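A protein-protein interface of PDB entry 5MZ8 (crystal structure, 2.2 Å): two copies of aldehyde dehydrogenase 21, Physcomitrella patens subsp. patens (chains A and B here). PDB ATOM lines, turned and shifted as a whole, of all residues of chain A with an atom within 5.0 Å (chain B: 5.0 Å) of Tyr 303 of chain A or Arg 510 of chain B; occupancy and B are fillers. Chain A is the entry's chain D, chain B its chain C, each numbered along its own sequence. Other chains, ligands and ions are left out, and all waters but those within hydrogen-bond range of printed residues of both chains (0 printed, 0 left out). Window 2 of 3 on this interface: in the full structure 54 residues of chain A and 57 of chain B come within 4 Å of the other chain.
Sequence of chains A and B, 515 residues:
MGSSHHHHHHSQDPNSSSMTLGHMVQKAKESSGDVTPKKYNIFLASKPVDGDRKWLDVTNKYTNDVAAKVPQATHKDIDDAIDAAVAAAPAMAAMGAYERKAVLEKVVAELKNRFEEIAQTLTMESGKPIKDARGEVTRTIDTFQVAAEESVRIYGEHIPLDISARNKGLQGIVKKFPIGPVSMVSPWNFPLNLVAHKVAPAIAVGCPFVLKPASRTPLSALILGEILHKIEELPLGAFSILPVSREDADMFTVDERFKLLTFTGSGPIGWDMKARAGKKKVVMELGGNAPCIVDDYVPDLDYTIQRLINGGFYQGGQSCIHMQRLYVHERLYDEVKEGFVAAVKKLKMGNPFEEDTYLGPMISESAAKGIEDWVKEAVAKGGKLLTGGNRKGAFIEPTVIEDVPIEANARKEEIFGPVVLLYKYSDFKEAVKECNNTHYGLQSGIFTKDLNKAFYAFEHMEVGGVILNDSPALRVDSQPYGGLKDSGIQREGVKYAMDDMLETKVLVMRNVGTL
OH of Tyr 303 of chain A touches CD of Arg 510 of chain B (3.1 Å). Arg 307 of chain A touches Arg 510 of chain B. CA of Met 509 of chain B touches O of Leu 468 of chain A (3.9 Å). Leu 468 of chain A touches Val 512 of chain B (CD2 to CG2, 3.95 Å). Asn 469 of chain A touches Arg 510 of chain B. Leu 170 of chain B touches Leu 474 of chain A (CD2 to CD2, 3.9 Å). Leu 474 of chain A touches Val 508 of chain B (CD2 to CG1, 3.8 Å). Leu 474 of chain A touches Arg 510 of chain B.
No position is printed for both chains.
Hydrophobic or aromatic side chains of chain B that line the printed part of chain A: Leu 170, Val 508 and Val 512. Along chain B the printed residues that touch a printed residue of chain A span positions 170 to 512. Along chain A the printed residues that touch a printed residue of chain B span positions 303 to 474. Among the printed residues, 11 pairs touch across the chains. Among the printed residues, Asp or Glu carboxylates within 4 Å of a Lys or Arg side-chain nitrogen of the other chain: Asp 470 of chain A with Arg 510 of chain B (2.8 Å).
N of Arg 510 of chain B lies within hydrogen-bond range of O of Leu 468 of chain A (3.1 Å). The backbone NH of Leu 468 of chain A lies within hydrogen-bond range of the backbone carbonyl oxygen of Val 508 of chain B (2.7 Å). NE of Arg 510 of chain B is in salt-bridge range of OD2 of Asp 470 of chain A.
Asp 302 of chain A touches none of the printed residues of chain B. Tyr 303 of chain A touches just one residue of chain B: Arg 510 (3.1 Å). Of the printed residues of chain B, Asn 469 of chain A touches Arg 510. Printed residues of chain B within 4 Å of Asp 470 of chain A: Arg 510 (2.8 Å). Of the printed residues of chain A, Met 509 of chain B touches Leu 468. Printed residues of chain A within 4 Å of Arg 510 of chain B: Tyr 303 (3.1 Å), Arg 307 (3.96 Å), Leu 468 (3.1 Å), Asn 469 (3.8 Å), Asp 470 (2.8 Å) and Leu 474 (3.6 Å). Of the printed residues of chain A, Val 512 of chain B touches Leu 468. The nearest printed residue of chain B that does not touch Arg 307 of chain A is Leu 170 of chain B (7.5 Å).
NH2 of Arg 307 of chain A is in salt-bridge range of OD2 of Asp 470 of chain A, at 2.8 Å. The side-chain carboxylate (OD1) of Asp 300 of chain A lies within hydrogen-bond range of the backbone NH (N) of Tyr 303 of chain A (3.0 Å).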
ATOM      1  N   VAL A 298     -16.434 -18.555  -9.354  1.00  0.00           N
ATOM      2  CA  VAL A 298     -17.620 -18.936  -8.568  1.00  0.00           C
ATOM      3  C   VAL A 298     -18.941 -18.723  -9.347  1.00  0.00           C
ATOM      4  O   VAL A 298     -19.307 -17.566  -9.575  1.00  0.00           O
ATOM      5  CB  VAL A 298     -17.684 -18.289  -7.143  1.00  0.00           C
ATOM      6  CG1 VAL A 298     -18.808 -18.916  -6.313  1.00  0.00           C
ATOM      7  CG2 VAL A 298     -16.351 -18.395  -6.400  1.00  0.00           C
ATOM      8  N   PRO A 299     -19.712 -19.799  -9.692  1.00  0.00           N
ATOM      9  CA  PRO A 299     -19.427 -21.236  -9.477  1.00  0.00           C
ATOM     10  C   PRO A 299     -18.455 -21.837 -10.497  1.00  0.00           C
ATOM     11  O   PRO A 299     -17.870 -22.884 -10.225  1.00  0.00           O
ATOM     12  CB  PRO A 299     -20.814 -21.876  -9.578  1.00  0.00           C
ATOM     13  CG  PRO A 299     -21.536 -21.009 -10.588  1.00  0.00           C
ATOM     14  CD  PRO A 299     -21.005 -19.607 -10.387  1.00  0.00           C
ATOM     15  N   ASP A 300     -18.303 -21.188 -11.678  1.00  0.00           N
ATOM     16  CA  ASP A 300     -17.423 -21.633 -12.755  1.00  0.00           C
ATOM     17  C   ASP A 300     -16.886 -20.449 -13.558  1.00  0.00           C
ATOM     18  O   ASP A 300     -17.302 -19.307 -13.333  1.00  0.00           O
ATOM     19  CB  ASP A 300     -18.120 -22.680 -13.656  1.00  0.00           C
ATOM     20  CG  ASP A 300     -19.488 -22.295 -14.194  1.00  0.00           C
ATOM     21  OD1 ASP A 300     -19.679 -21.115 -14.549  1.00  0.00           O
ATOM     22  OD2 ASP A 300     -20.349 -23.188 -14.310  1.00  0.00           O
ATOM     23  N   LEU A 301     -15.944 -20.723 -14.480  1.00  0.00           N
ATOM     24  CA  LEU A 301     -15.316 -19.690 -15.315  1.00  0.00           C
ATOM     25  C   LEU A 301     -16.314 -18.928 -16.168  1.00  0.00           C
ATOM     26  O   LEU A 301     -16.271 -17.703 -16.196  1.00  0.00           O
ATOM     27  CB  LEU A 301     -14.177 -20.277 -16.177  1.00  0.00           C
ATOM     28  CG  LEU A 301     -13.398 -19.288 -17.058  1.00  0.00           C
ATOM     29  CD1 LEU A 301     -12.685 -18.232 -16.230  1.00  0.00           C
ATOM     30  CD2 LEU A 301     -12.426 -20.026 -17.959  1.00  0.00           C
ATOM     31  N   ASP A 302     -17.227 -19.652 -16.834  1.00  0.00           N
ATOM     32  CA  ASP A 302     -18.248 -19.067 -17.706  1.00  0.00           C
ATOM     33  C   ASP A 302     -19.103 -18.030 -16.984  1.00  0.00           C
ATOM     34  O   ASP A 302     -19.236 -16.919 -17.484  1.00  0.00           O
ATOM     35  CB  ASP A 302     -19.098 -20.154 -18.389  1.00  0.00           C
ATOM     36  CG  ASP A 302     -18.368 -20.954 -19.468  1.00  0.00           C
ATOM     37  OD1 ASP A 302     -17.205 -20.595 -19.805  1.00  0.00           O
ATOM     38  OD2 ASP A 302     -18.957 -21.935 -19.981  1.00  0.00           O
ATOM     39  N   TYR A 303     -19.607 -18.364 -15.781  1.00  0.00           N
ATOM     40  CA  TYR A 303     -20.397 -17.434 -14.979  1.00  0.00           C
ATOM     41  C   TYR A 303     -19.549 -16.254 -14.471  1.00  0.00           C
ATOM     42  O   TYR A 303     -20.052 -15.131 -14.436  1.00  0.00           O
ATOM     43  CB  TYR A 303     -21.125 -18.140 -13.827  1.00  0.00           C
ATOM     44  CG  TYR A 303     -22.120 -17.232 -13.133  1.00  0.00           C
ATOM     45  CD1 TYR A 303     -23.363 -16.961 -13.702  1.00  0.00           C
ATOM     46  CD2 TYR A 303     -21.801 -16.604 -11.927  1.00  0.00           C
ATOM     47  CE1 TYR A 303     -24.282 -16.123 -13.067  1.00  0.00           C
ATOM     48  CE2 TYR A 303     -22.720 -15.777 -11.276  1.00  0.00           C
ATOM     49  CZ  TYR A 303     -23.953 -15.528 -11.859  1.00  0.00           C
ATOM     50  OH  TYR A 303     -24.851 -14.691 -11.252  1.00  0.00           O
ATOM     51  N   THR A 304     -18.263 -16.513 -14.102  1.00  0.00           N
ATOM     52  CA  THR A 304     -17.322 -15.481 -13.648  1.00  0.00           C
ATOM     53  C   THR A 304     -17.086 -14.466 -14.774  1.00  0.00           C
ATOM     54  O   THR A 304     -17.280 -13.281 -14.535  1.00  0.00           O
ATOM     55  CB  THR A 304     -16.022 -16.091 -13.091  1.00  0.00           C
ATOM     56  OG1 THR A 304     -16.350 -17.052 -12.094  1.00  0.00           O
ATOM     57  CG2 THR A 304     -15.098 -15.041 -12.491  1.00  0.00           C
ATOM     58  N   ILE A 305     -16.742 -14.930 -16.003  1.00  0.00           N
ATOM     59  CA  ILE A 305     -16.524 -14.062 -17.176  1.00  0.00           C
ATOM     60  C   ILE A 305     -17.767 -13.194 -17.453  1.00  0.00           C
ATOM     61  O   ILE A 305     -17.648 -11.990 -17.619  1.00  0.00           O
ATOM     62  CB  ILE A 305     -16.042 -14.861 -18.439  1.00  0.00           C
ATOM     63  CG1 ILE A 305     -14.669 -15.577 -18.223  1.00  0.00           C
ATOM     64  CG2 ILE A 305     -16.028 -13.994 -19.719  1.00  0.00           C
ATOM     65  CD1 ILE A 305     -13.442 -14.712 -17.838  1.00  0.00           C
ATOM     66  N   GLN A 306     -18.939 -13.807 -17.439  1.00  0.00           N
ATOM     67  CA  GLN A 306     -20.241 -13.183 -17.665  1.00  0.00           C
ATOM     68  C   GLN A 306     -20.492 -12.003 -16.700  1.00  0.00           C
ATOM     69  O   GLN A 306     -20.929 -10.940 -17.136  1.00  0.00           O
ATOM     70  CB  GLN A 306     -21.300 -14.270 -17.471  1.00  0.00           C
ATOM     71  CG  GLN A 306     -22.615 -14.068 -18.190  1.00  0.00           C
ATOM     72  CD  GLN A 306     -23.571 -15.151 -17.745  1.00  0.00           C
ATOM     73  OE1 GLN A 306     -23.522 -16.289 -18.231  1.00  0.00           O
ATOM     74  NE2 GLN A 306     -24.379 -14.854 -16.726  1.00  0.00           N
ATOM     75  N   ARG A 307     -20.187 -12.192 -15.398  1.00  0.00           N
ATOM     76  CA  ARG A 307     -20.356 -11.182 -14.347  1.00  0.00           C
ATOM     77  C   ARG A 307     -19.296 -10.105 -14.442  1.00  0.00           C
ATOM     78  O   ARG A 307     -19.579  -8.951 -14.125  1.00  0.00           O
ATOM     79  CB  ARG A 307     -20.342 -11.836 -12.952  1.00  0.00           C
ATOM     80  CG  ARG A 307     -21.452 -12.851 -12.730  1.00  0.00           C
ATOM     81  CD  ARG A 307     -22.744 -12.228 -12.250  1.00  0.00           C
ATOM     82  NE  ARG A 307     -23.568 -11.730 -13.341  1.00  0.00           N
ATOM     83  CZ  ARG A 307     -24.367 -10.673 -13.251  1.00  0.00           C
ATOM     84  NH1 ARG A 307     -25.090 -10.292 -14.293  1.00  0.00           N
ATOM     85  NH2 ARG A 307     -24.443  -9.982 -12.120  1.00  0.00           N
ATOM     86  N   LEU A 468     -19.828  -9.964  -2.934  1.00  0.00           N
ATOM     87  CA  LEU A 468     -19.294 -11.318  -2.810  1.00  0.00           C
ATOM     88  C   LEU A 468     -19.834 -12.239  -3.893  1.00  0.00           C
ATOM     89  O   LEU A 468     -21.038 -12.478  -3.974  1.00  0.00           O
ATOM     90  CB  LEU A 468     -19.529 -11.885  -1.395  1.00  0.00           C
ATOM     91  CG  LEU A 468     -18.971 -13.293  -1.045  1.00  0.00           C
ATOM     92  CD1 LEU A 468     -17.470 -13.453  -1.375  1.00  0.00           C
ATOM     93  CD2 LEU A 468     -19.222 -13.607   0.399  1.00  0.00           C
ATOM     94  N   ASN A 469     -18.909 -12.714  -4.738  1.00  0.00           N
ATOM     95  CA  ASN A 469     -19.091 -13.637  -5.854  1.00  0.00           C
ATOM     96  C   ASN A 469     -19.990 -13.058  -6.954  1.00  0.00           C
ATOM     97  O   ASN A 469     -20.830 -13.749  -7.550  1.00  0.00           O
ATOM     98  CB  ASN A 469     -19.517 -15.031  -5.366  1.00  0.00           C
ATOM     99  CG  ASN A 469     -18.382 -15.703  -4.638  1.00  0.00           C
ATOM    100  OD1 ASN A 469     -17.202 -15.453  -4.915  1.00  0.00           O
ATOM    101  ND2 ASN A 469     -18.693 -16.555  -3.689  1.00  0.00           N
ATOM    102  N   ASP A 470     -19.740 -11.767  -7.229  1.00  0.00           N
ATOM    103  CA  ASP A 470     -20.276 -10.927  -8.294  1.00  0.00           C
ATOM    104  C   ASP A 470     -19.361  -9.697  -8.383  1.00  0.00           C
ATOM    105  O   ASP A 470     -18.593  -9.432  -7.444  1.00  0.00           O
ATOM    106  CB  ASP A 470     -21.769 -10.564  -8.111  1.00  0.00           C
ATOM    107  CG  ASP A 470     -22.513 -10.217  -9.405  1.00  0.00           C
ATOM    108  OD1 ASP A 470     -21.842  -9.917 -10.427  1.00  0.00           O
ATOM    109  OD2 ASP A 470     -23.761 -10.207  -9.388  1.00  0.00           O
ATOM    110  N   LEU A 474     -23.046  -4.516  -8.997  1.00  0.00           N
ATOM    111  CA  LEU A 474     -24.321  -4.993  -8.472  1.00  0.00           C
ATOM    112  C   LEU A 474     -24.899  -4.066  -7.399  1.00  0.00           C
ATOM    113  O   LEU A 474     -24.216  -3.738  -6.422  1.00  0.00           O
ATOM    114  CB  LEU A 474     -24.162  -6.427  -7.919  1.00  0.00           C
ATOM    115  CG  LEU A 474     -25.412  -7.101  -7.355  1.00  0.00           C
ATOM    116  CD1 LEU A 474     -26.426  -7.405  -8.470  1.00  0.00           C
ATOM    117  CD2 LEU A 474     -25.059  -8.354  -6.624  1.00  0.00           C
ATOM    118  N   LYS B 168     -32.938 -12.681  -7.219  1.00  0.00           N
ATOM    119  CA  LYS B 168     -32.896 -14.063  -6.738  1.00  0.00           C
ATOM    120  C   LYS B 168     -31.468 -14.447  -6.266  1.00  0.00           C
ATOM    121  O   LYS B 168     -30.482 -14.075  -6.912  1.00  0.00           O
ATOM    122  CB  LYS B 168     -33.372 -14.999  -7.868  1.00  0.00           C
ATOM    123  CG  LYS B 168     -33.171 -16.501  -7.621  1.00  0.00           C
ATOM    124  CD  LYS B 168     -33.921 -17.384  -8.592  1.00  0.00           C
ATOM    125  CE  LYS B 168     -33.188 -17.793  -9.859  1.00  0.00           C
ATOM    126  NZ  LYS B 168     -33.167 -16.698 -10.872  1.00  0.00           N
ATOM    127  N   GLY B 169     -31.390 -15.163  -5.144  1.00  0.00           N
ATOM    128  CA  GLY B 169     -30.148 -15.669  -4.579  1.00  0.00           C
ATOM    129  C   GLY B 169     -29.264 -14.643  -3.908  1.00  0.00           C
ATOM    130  O   GLY B 169     -28.080 -14.916  -3.687  1.00  0.00           O
ATOM    131  N   LEU B 170     -29.835 -13.467  -3.549  1.00  0.00           N
ATOM    132  CA  LEU B 170     -29.076 -12.399  -2.904  1.00  0.00           C
ATOM    133  C   LEU B 170     -29.498 -12.182  -1.461  1.00  0.00           C
ATOM    134  O   LEU B 170     -30.681 -12.210  -1.134  1.00  0.00           O
ATOM    135  CB  LEU B 170     -29.146 -11.080  -3.682  1.00  0.00           C
ATOM    136  CG  LEU B 170     -28.638 -11.086  -5.146  1.00  0.00           C
ATOM    137  CD1 LEU B 170     -28.953  -9.777  -5.833  1.00  0.00           C
ATOM    138  CD2 LEU B 170     -27.131 -11.346  -5.225  1.00  0.00           C
ATOM    139  N   VAL B 508     -22.808  -7.838   0.085  1.00  0.00           N
ATOM    140  CA  VAL B 508     -23.878  -8.370  -0.767  1.00  0.00           C
ATOM    141  C   VAL B 508     -23.386  -9.726  -1.256  1.00  0.00           C
ATOM    142  O   VAL B 508     -22.336  -9.811  -1.889  1.00  0.00           O
ATOM    143  CB  VAL B 508     -24.318  -7.414  -1.917  1.00  0.00           C
ATOM    144  CG1 VAL B 508     -25.379  -8.065  -2.806  1.00  0.00           C
ATOM    145  CG2 VAL B 508     -24.817  -6.075  -1.360  1.00  0.00           C
ATOM    146  N   MET B 509     -24.112 -10.786  -0.900  1.00  0.00           N
ATOM    147  CA  MET B 509     -23.706 -12.168  -1.135  1.00  0.00           C
ATOM    148  C   MET B 509     -24.559 -12.850  -2.168  1.00  0.00           C
ATOM    149  O   MET B 509     -25.773 -12.971  -1.975  1.00  0.00           O
ATOM    150  CB  MET B 509     -23.738 -12.947   0.186  1.00  0.00           C
ATOM    151  CG  MET B 509     -23.014 -12.253   1.330  1.00  0.00           C
ATOM    152  SD  MET B 509     -23.585 -12.839   2.943  1.00  0.00           S
ATOM    153  CE  MET B 509     -22.641 -14.323   3.071  1.00  0.00           C
ATOM    154  N   ARG B 510     -23.920 -13.290  -3.275  1.00  0.00           N
ATOM    155  CA  ARG B 510     -24.595 -13.989  -4.368  1.00  0.00           C
ATOM    156  C   ARG B 510     -24.434 -15.498  -4.235  1.00  0.00           C
ATOM    157  O   ARG B 510     -23.310 -16.015  -4.316  1.00  0.00           O
ATOM    158  CB  ARG B 510     -24.138 -13.514  -5.764  1.00  0.00           C
ATOM    159  CG  ARG B 510     -24.917 -14.232  -6.868  1.00  0.00           C
ATOM    160  CD  ARG B 510     -24.643 -13.748  -8.266  1.00  0.00           C
ATOM    161  NE  ARG B 510     -25.214 -12.426  -8.566  1.00  0.00           N
ATOM    162  CZ  ARG B 510     -26.492 -12.183  -8.864  1.00  0.00           C
ATOM    163  NH1 ARG B 510     -27.388 -13.160  -8.833  1.00  0.00           N
ATOM    164  NH2 ARG B 510     -26.887 -10.953  -9.158  1.00  0.00           N
ATOM    165  N   ASN B 511     -25.574 -16.192  -4.065  1.00  0.00           N
ATOM    166  CA  ASN B 511     -25.690 -17.649  -3.932  1.00  0.00           C
ATOM    167  C   ASN B 511     -24.698 -18.255  -2.921  1.00  0.00           C
ATOM    168  O   ASN B 511     -24.110 -19.299  -3.183  1.00  0.00           O
ATOM    169  CB  ASN B 511     -25.620 -18.347  -5.299  1.00  0.00           C
ATOM    170  CG  ASN B 511     -26.717 -17.937  -6.252  1.00  0.00           C
ATOM    171  OD1 ASN B 511     -27.916 -17.993  -5.934  1.00  0.00           O
ATOM    172  ND2 ASN B 511     -26.320 -17.500  -7.446  1.00  0.00           N
ATOM    173  N   VAL B 512     -24.523 -17.592  -1.761  1.00  0.00           N
ATOM    174  CA  VAL B 512     -23.631 -18.091  -0.712  1.00  0.00           C
ATOM    175  C   VAL B 512     -24.374 -19.194   0.074  1.00  0.00           C
ATOM    176  O   VAL B 512     -25.481 -18.970   0.582  1.00  0.00           O
ATOM    177  CB  VAL B 512     -23.019 -16.962   0.159  1.00  0.00           C
ATOM    178  CG1 VAL B 512     -22.222 -17.537   1.321  1.00  0.00           C
ATOM    179  CG2 VAL B 512     -22.125 -16.061  -0.691  1.00  0.00           C
